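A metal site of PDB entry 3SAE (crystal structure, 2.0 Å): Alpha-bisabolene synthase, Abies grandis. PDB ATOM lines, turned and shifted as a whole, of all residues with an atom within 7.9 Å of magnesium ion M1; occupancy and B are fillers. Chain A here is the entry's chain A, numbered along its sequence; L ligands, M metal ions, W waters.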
ATOM      1  N   TYR A 659      31.117  17.541  23.577  1.00  0.00           N
ATOM      2  CA  TYR A 659      30.318  16.552  22.862  1.00  0.00           C
ATOM      3  C   TYR A 659      30.839  15.150  23.109  1.00  0.00           C
ATOM      4  O   TYR A 659      30.079  14.219  23.374  1.00  0.00           O
ATOM      5  CB  TYR A 659      30.331  16.873  21.374  1.00  0.00           C
ATOM      6  CG  TYR A 659      29.646  15.830  20.494  1.00  0.00           C
ATOM      7  CD1 TYR A 659      28.298  15.937  20.178  1.00  0.00           C
ATOM      8  CD2 TYR A 659      30.360  14.759  19.967  1.00  0.00           C
ATOM      9  CE1 TYR A 659      27.674  14.997  19.372  1.00  0.00           C
ATOM     10  CE2 TYR A 659      29.736  13.809  19.162  1.00  0.00           C
ATOM     11  CZ  TYR A 659      28.402  13.938  18.860  1.00  0.00           C
ATOM     12  OH  TYR A 659      27.792  13.001  18.071  1.00  0.00           O
ATOM     13  N   SER A 709      32.433   3.949  19.339  1.00  0.00           N
ATOM     14  CA  SER A 709      31.053   3.845  18.908  1.00  0.00           C
ATOM     15  C   SER A 709      30.479   5.216  18.523  1.00  0.00           C
ATOM     16  O   SER A 709      29.899   5.369  17.453  1.00  0.00           O
ATOM     17  CB  SER A 709      30.199   3.201  20.005  1.00  0.00           C
ATOM     18  OG  SER A 709      30.610   1.859  20.259  1.00  0.00           O
ATOM     19  N   ARG A 710      30.629   6.191  19.407  1.00  0.00           N
ATOM     20  CA  ARG A 710      30.136   7.542  19.151  1.00  0.00           C
ATOM     21  C   ARG A 710      30.704   8.131  17.851  1.00  0.00           C
ATOM     22  O   ARG A 710      29.957   8.639  16.996  1.00  0.00           O
ATOM     23  CB  ARG A 710      30.469   8.463  20.332  1.00  0.00           C
ATOM     24  CG  ARG A 710      30.114   9.945  20.126  1.00  0.00           C
ATOM     25  CD  ARG A 710      28.607  10.167  20.123  1.00  0.00           C
ATOM     26  NE  ARG A 710      27.987   9.680  18.902  1.00  0.00           N
ATOM     27  CZ  ARG A 710      26.689   9.466  18.738  1.00  0.00           C
ATOM     28  NH1 ARG A 710      25.842   9.707  19.738  1.00  0.00           N
ATOM     29  NH2 ARG A 710      26.227   9.021  17.577  1.00  0.00           N
ATOM     30  N   LEU A 711      32.013   8.065  17.701  1.00  0.00           N
ATOM     31  CA  LEU A 711      32.689   8.678  16.549  1.00  0.00           C
ATOM     32  C   LEU A 711      32.508   7.884  15.259  1.00  0.00           C
ATOM     33  O   LEU A 711      32.298   8.458  14.191  1.00  0.00           O
ATOM     34  CB  LEU A 711      34.165   8.906  16.854  1.00  0.00           C
ATOM     35  CG  LEU A 711      34.441   9.927  17.961  1.00  0.00           C
ATOM     36  CD1 LEU A 711      35.940  10.161  18.104  1.00  0.00           C
ATOM     37  CD2 LEU A 711      33.718  11.242  17.693  1.00  0.00           C
ATOM     38  N   ALA A 712      32.561   6.553  15.348  1.00  0.00           N
ATOM     39  CA  ALA A 712      32.294   5.734  14.176  1.00  0.00           C
ATOM     40  C   ALA A 712      30.878   5.985  13.688  1.00  0.00           C
ATOM     41  O   ALA A 712      30.649   6.155  12.490  1.00  0.00           O
ATOM     42  CB  ALA A 712      32.507   4.256  14.478  1.00  0.00           C
ATOM     43  N   ASP A 713      29.938   6.032  14.615  1.00  0.00           N
ATOM     44  CA  ASP A 713      28.573   6.373  14.247  1.00  0.00           C
ATOM     45  C   ASP A 713      28.540   7.733  13.546  1.00  0.00           C
ATOM     46  O   ASP A 713      27.948   7.866  12.471  1.00  0.00           O
ATOM     47  CB  ASP A 713      27.650   6.384  15.467  1.00  0.00           C
ATOM     48  CG  ASP A 713      26.277   6.922  15.133  1.00  0.00           C
ATOM     49  OD1 ASP A 713      26.133   8.163  15.058  1.00  0.00           O
ATOM     50  OD2 ASP A 713      25.332   6.123  14.954  1.00  0.00           O
ATOM     51  N   ASP A 714      29.167   8.742  14.143  1.00  0.00           N
ATOM     52  CA  ASP A 714      29.168  10.077  13.541  1.00  0.00           C
ATOM     53  C   ASP A 714      29.690  10.059  12.107  1.00  0.00           C
ATOM     54  O   ASP A 714      29.092  10.666  11.221  1.00  0.00           O
ATOM     55  CB  ASP A 714      29.987  11.066  14.386  1.00  0.00           C
ATOM     56  CG  ASP A 714      29.296  11.445  15.681  1.00  0.00           C
ATOM     57  OD1 ASP A 714      28.131  11.025  15.881  1.00  0.00           O
ATOM     58  OD2 ASP A 714      29.917  12.153  16.493  1.00  0.00           O
ATOM     59  N   THR A 715      30.803   9.353  11.885  1.00  0.00           N
ATOM     60  CA  THR A 715      31.413   9.282  10.563  1.00  0.00           C
ATOM     61  C   THR A 715      30.500   8.601   9.557  1.00  0.00           C
ATOM     62  O   THR A 715      30.592   8.856   8.362  1.00  0.00           O
ATOM     63  CB  THR A 715      32.758   8.514  10.586  1.00  0.00           C
ATOM     64  OG1 THR A 715      32.522   7.171  11.018  1.00  0.00           O
ATOM     65  CG2 THR A 715      33.737   9.186  11.526  1.00  0.00           C
ATOM     66  N   LYS A 716      29.643   7.715  10.057  1.00  0.00           N
ATOM     67  CA  LYS A 716      28.752   6.955   9.194  1.00  0.00           C
ATOM     68  C   LYS A 716      27.421   7.667   8.936  1.00  0.00           C
ATOM     69  O   LYS A 716      26.741   7.369   7.961  1.00  0.00           O
ATOM     70  CB  LYS A 716      28.468   5.579   9.818  1.00  0.00           C
ATOM     71  CG  LYS A 716      27.677   4.623   8.919  1.00  0.00           C
ATOM     72  CD  LYS A 716      28.489   4.227   7.702  1.00  0.00           C
ATOM     73  CE  LYS A 716      27.863   3.063   6.952  1.00  0.00           C
ATOM     74  NZ  LYS A 716      28.664   2.766   5.722  1.00  0.00           N
ATOM     75  N   THR A 717      27.053   8.603   9.806  1.00  0.00           N
ATOM     76  CA  THR A 717      25.675   9.096   9.844  1.00  0.00           C
ATOM     77  C   THR A 717      25.466  10.623   9.856  1.00  0.00           C
ATOM     78  O   THR A 717      24.345  11.091   9.638  1.00  0.00           O
ATOM     79  CB  THR A 717      24.890   8.510  11.050  1.00  0.00           C
ATOM     80  OG1 THR A 717      25.595   8.794  12.261  1.00  0.00           O
ATOM     81  CG2 THR A 717      24.748   7.009  10.901  1.00  0.00           C
ATOM     82  N   TYR A 718      26.512  11.395  10.119  1.00  0.00           N
ATOM     83  CA  TYR A 718      26.327  12.826  10.368  1.00  0.00           C
ATOM     84  C   TYR A 718      25.660  13.604   9.223  1.00  0.00           C
ATOM     85  O   TYR A 718      25.039  14.652   9.450  1.00  0.00           O
ATOM     86  CB  TYR A 718      27.665  13.487  10.744  1.00  0.00           C
ATOM     87  CG  TYR A 718      28.509  13.853   9.548  1.00  0.00           C
ATOM     88  CD1 TYR A 718      29.266  12.894   8.889  1.00  0.00           C
ATOM     89  CD2 TYR A 718      28.538  15.157   9.068  1.00  0.00           C
ATOM     90  CE1 TYR A 718      30.042  13.234   7.796  1.00  0.00           C
ATOM     91  CE2 TYR A 718      29.302  15.496   7.968  1.00  0.00           C
ATOM     92  CZ  TYR A 718      30.056  14.531   7.342  1.00  0.00           C
ATOM     93  OH  TYR A 718      30.820  14.860   6.244  1.00  0.00           O
ATOM     94  N   LYS A 719      25.778  13.096   7.994  1.00  0.00           N
ATOM     95  CA  LYS A 719      25.263  13.825   6.840  1.00  0.00           C
ATOM     96  C   LYS A 719      23.751  13.688   6.675  1.00  0.00           C
ATOM     97  O   LYS A 719      23.075  14.643   6.295  1.00  0.00           O
ATOM     98  CB  LYS A 719      25.986  13.407   5.555  1.00  0.00           C
ATOM     99  CG  LYS A 719      27.471  13.695   5.589  1.00  0.00           C
ATOM    100  CD  LYS A 719      27.887  14.645   4.478  1.00  0.00           C
ATOM    101  CE  LYS A 719      27.911  13.936   3.136  1.00  0.00           C
ATOM    102  NZ  LYS A 719      28.997  12.911   3.084  1.00  0.00           N
ATOM    103  N   ALA A 720      23.217  12.502   6.966  1.00  0.00           N
ATOM    104  CA  ALA A 720      21.770  12.308   6.950  1.00  0.00           C
ATOM    105  C   ALA A 720      21.139  13.116   8.070  1.00  0.00           C
ATOM    106  O   ALA A 720      20.055  13.695   7.909  1.00  0.00           O
ATOM    107  CB  ALA A 720      21.424  10.840   7.105  1.00  0.00           C
ATOM    108  N   GLU A 721      21.822  13.166   9.208  1.00  0.00           N
ATOM    109  CA  GLU A 721      21.345  13.893  10.376  1.00  0.00           C
ATOM    110  C   GLU A 721      21.413  15.390  10.169  1.00  0.00           C
ATOM    111  O   GLU A 721      20.527  16.123  10.613  1.00  0.00           O
ATOM    112  CB  GLU A 721      22.172  13.503  11.599  1.00  0.00           C
ATOM    113  CG  GLU A 721      22.097  12.026  11.940  1.00  0.00           C
ATOM    114  CD  GLU A 721      23.218  11.582  12.851  1.00  0.00           C
ATOM    115  OE1 GLU A 721      23.230  10.396  13.229  1.00  0.00           O
ATOM    116  OE2 GLU A 721      24.086  12.422  13.177  1.00  0.00           O
ATOM    117  N   ARG A 724      18.516  16.261   7.894  1.00  0.00           N
ATOM    118  CA  ARG A 724      17.251  16.224   8.631  1.00  0.00           C
ATOM    119  C   ARG A 724      17.104  17.409   9.586  1.00  0.00           C
ATOM    120  O   ARG A 724      16.016  17.683  10.087  1.00  0.00           O
ATOM    121  CB  ARG A 724      17.127  14.930   9.444  1.00  0.00           C
ATOM    122  CG  ARG A 724      17.185  13.646   8.641  1.00  0.00           C
ATOM    123  CD  ARG A 724      16.726  12.476   9.504  1.00  0.00           C
ATOM    124  NE  ARG A 724      17.314  11.204   9.070  1.00  0.00           N
ATOM    125  CZ  ARG A 724      18.288  10.577   9.723  1.00  0.00           C
ATOM    126  NH1 ARG A 724      18.789  11.096  10.832  1.00  0.00           N
ATOM    127  NH2 ARG A 724      18.757   9.431   9.256  1.00  0.00           N
ATOM    128  N   GLU A 726      18.986  17.624  12.376  1.00  0.00           N
ATOM    129  CA  GLU A 726      19.302  17.122  13.709  1.00  0.00           C
ATOM    130  C   GLU A 726      20.346  17.954  14.431  1.00  0.00           C
ATOM    131  O   GLU A 726      21.099  18.719  13.808  1.00  0.00           O
ATOM    132  CB  GLU A 726      19.768  15.662  13.645  1.00  0.00           C
ATOM    133  CG  GLU A 726      18.747  14.655  14.162  1.00  0.00           C
ATOM    134  CD  GLU A 726      19.273  13.221  14.132  1.00  0.00           C
ATOM    135  OE1 GLU A 726      20.349  12.958  14.704  1.00  0.00           O
ATOM    136  OE2 GLU A 726      18.595  12.361  13.524  1.00  0.00           O
ATOM    137  N   SER A 729      26.581  16.922  15.416  1.00  0.00           N
ATOM    138  CA  SER A 729      27.418  15.774  15.714  1.00  0.00           C
ATOM    139  C   SER A 729      28.850  16.239  15.983  1.00  0.00           C
ATOM    140  O   SER A 729      29.103  17.445  16.110  1.00  0.00           O
ATOM    141  CB  SER A 729      27.418  14.823  14.508  1.00  0.00           C
ATOM    142  OG  SER A 729      28.028  15.439  13.382  1.00  0.00           O
ATOM    143  N   PHE A 790      29.160   0.437  11.404  1.00  0.00           N
ATOM    144  CA  PHE A 790      29.534   1.808  11.070  1.00  0.00           C
ATOM    145  C   PHE A 790      30.743   1.925  10.136  1.00  0.00           C
ATOM    146  O   PHE A 790      31.316   3.011   9.976  1.00  0.00           O
ATOM    147  CB  PHE A 790      29.775   2.593  12.357  1.00  0.00           C
ATOM    148  CG  PHE A 790      28.581   2.642  13.252  1.00  0.00           C
ATOM    149  CD1 PHE A 790      27.342   3.036  12.762  1.00  0.00           C
ATOM    150  CD2 PHE A 790      28.683   2.288  14.582  1.00  0.00           C
ATOM    151  CE1 PHE A 790      26.233   3.076  13.585  1.00  0.00           C
ATOM    152  CE2 PHE A 790      27.565   2.328  15.408  1.00  0.00           C
ATOM    153  CZ  PHE A 790      26.343   2.720  14.903  1.00  0.00           C
ATOM    154  N   GLY A 795      28.921   9.169   5.762  1.00  0.00           N
ATOM    155  CA  GLY A 795      28.038  10.125   6.410  1.00  0.00           C
ATOM    156  C   GLY A 795      26.576   9.943   6.073  1.00  0.00           C
ATOM    157  O   GLY A 795      25.703  10.524   6.714  1.00  0.00           O
ATOM    158  N   GLY A 797      24.522   7.318   6.288  1.00  0.00           N
ATOM    159  CA  GLY A 797      23.724   6.572   7.241  1.00  0.00           C
ATOM    160  C   GLY A 797      24.042   5.094   7.206  1.00  0.00           C
ATOM    161  O   GLY A 797      24.794   4.630   6.347  1.00  0.00           O
ATOM    162  N   VAL A 798      23.477   4.349   8.144  1.00  0.00           N
ATOM    163  CA  VAL A 798      23.689   2.907   8.223  1.00  0.00           C
ATOM    164  C   VAL A 798      22.779   2.178   7.234  1.00  0.00           C
ATOM    165  O   VAL A 798      21.623   2.560   7.048  1.00  0.00           O
ATOM    166  CB  VAL A 798      23.451   2.392   9.650  1.00  0.00           C
ATOM    167  CG1 VAL A 798      23.294   0.863   9.654  1.00  0.00           C
ATOM    168  CG2 VAL A 798      24.565   2.839  10.570  1.00  0.00           C
HETATM  169  C1  LIG L   1      23.041   5.815  19.528  1.00  0.00           C
HETATM  170  S1  LIG L   1      22.327   6.431  17.982  1.00  0.00           S
HETATM  171  C2  LIG L   1      23.309   4.328  19.371  1.00  0.00           C
HETATM  172  C3  LIG L   1      24.424   3.886  18.827  1.00  0.00           C
HETATM  173  C4  LIG L   1      25.469   4.857  18.331  1.00  0.00           C
HETATM  174  C5  LIG L   1      24.625   2.398  18.603  1.00  0.00           C
HETATM  175  C6  LIG L   1      25.762   1.902  19.498  1.00  0.00           C
HETATM  176  C7  LIG L   1      25.392   2.136  20.945  1.00  0.00           C
HETATM  177  C8  LIG L   1      24.871   1.165  21.658  1.00  0.00           C
HETATM  178  C9  LIG L   1      24.525   1.402  23.119  1.00  0.00           C
HETATM  179  C10 LIG L   1      24.826  -0.228  21.083  1.00  0.00           C
HETATM  180  C11 LIG L   1      23.037   1.157  23.371  1.00  0.00           C
HETATM  181  C12 LIG L   1      22.205   2.299  22.833  1.00  0.00           C
HETATM  182  C13 LIG L   1      21.172   2.046  22.060  1.00  0.00           C
HETATM  183  C14 LIG L   1      20.481   3.172  21.335  1.00  0.00           C
HETATM  184  C15 LIG L   1      20.808   0.615  21.787  1.00  0.00           C
HETATM  185  P1  LIG L   1      22.024   8.458  18.501  1.00  0.00           P
HETATM  186  O1  LIG L   1      20.804   8.603  19.366  1.00  0.00           O
HETATM  187  O2  LIG L   1      23.270   9.009  19.364  1.00  0.00           O
HETATM  188  O3  LIG L   1      21.830   9.269  17.133  1.00  0.00           O
HETATM  189 MG    MG M   1      24.648   9.264  14.113  1.00  0.00          MG
HETATM  190 MG    MG M   2      18.789   8.391  19.084  1.00  0.00          MG
HETATM  191  O   HOH W   1      25.969  10.865  14.285  1.00  0.00           O
HETATM  192  O   HOH W   2      24.035   9.947  16.007  1.00  0.00           O
HETATM  193  O   HOH W   3      23.340   7.647  14.169  1.00  0.00           O
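The guanidinium group of Arg 710 sits at hydrogen-bond distance from the side-chain hydroxyl of Tyr 659 (3.4 Å). The side-chain carboxylate of Asp 713 lies close to the guanidinium group of Arg 710, 2.7 Å away. OD1 of Asp 714 is in salt-bridge range of NH2 of Arg 710 (3.2 Å). The backbone carbonyl oxygen (O) of Glu 721 sits at hydrogen-bond distance from the backbone NH (N) of Glu 726 (2.8 Å).
Water W2 lies within hydrogen-bond range of O3 of the ligand (2.6 Å) and NH2 of Arg 710 (2.9 Å). Water W1 bridges OE2 of Glu 721 (2.7 Å) and OD1 of Asp 714 (2.7 Å).
The guanidinium group (NH1) of Arg 710 lies within salt-bridge range of an oxygen (O2) of the ligand (2.7 Å).
Magnesium ion M1 is bound by OE1 of Glu 721 (2.0 Å), OD1 of Asp 713 (2.1 Å), water W3 (2.1 Å), water W1 (2.1 Å), water W2 (2.1 Å) and OG1 of Thr 717 (2.1 Å). Magnesium ion M1 has six donor atoms within binding distance.
Arg 710 touches magnesium ion M1 (NH2 to MG, 3.8 Å).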
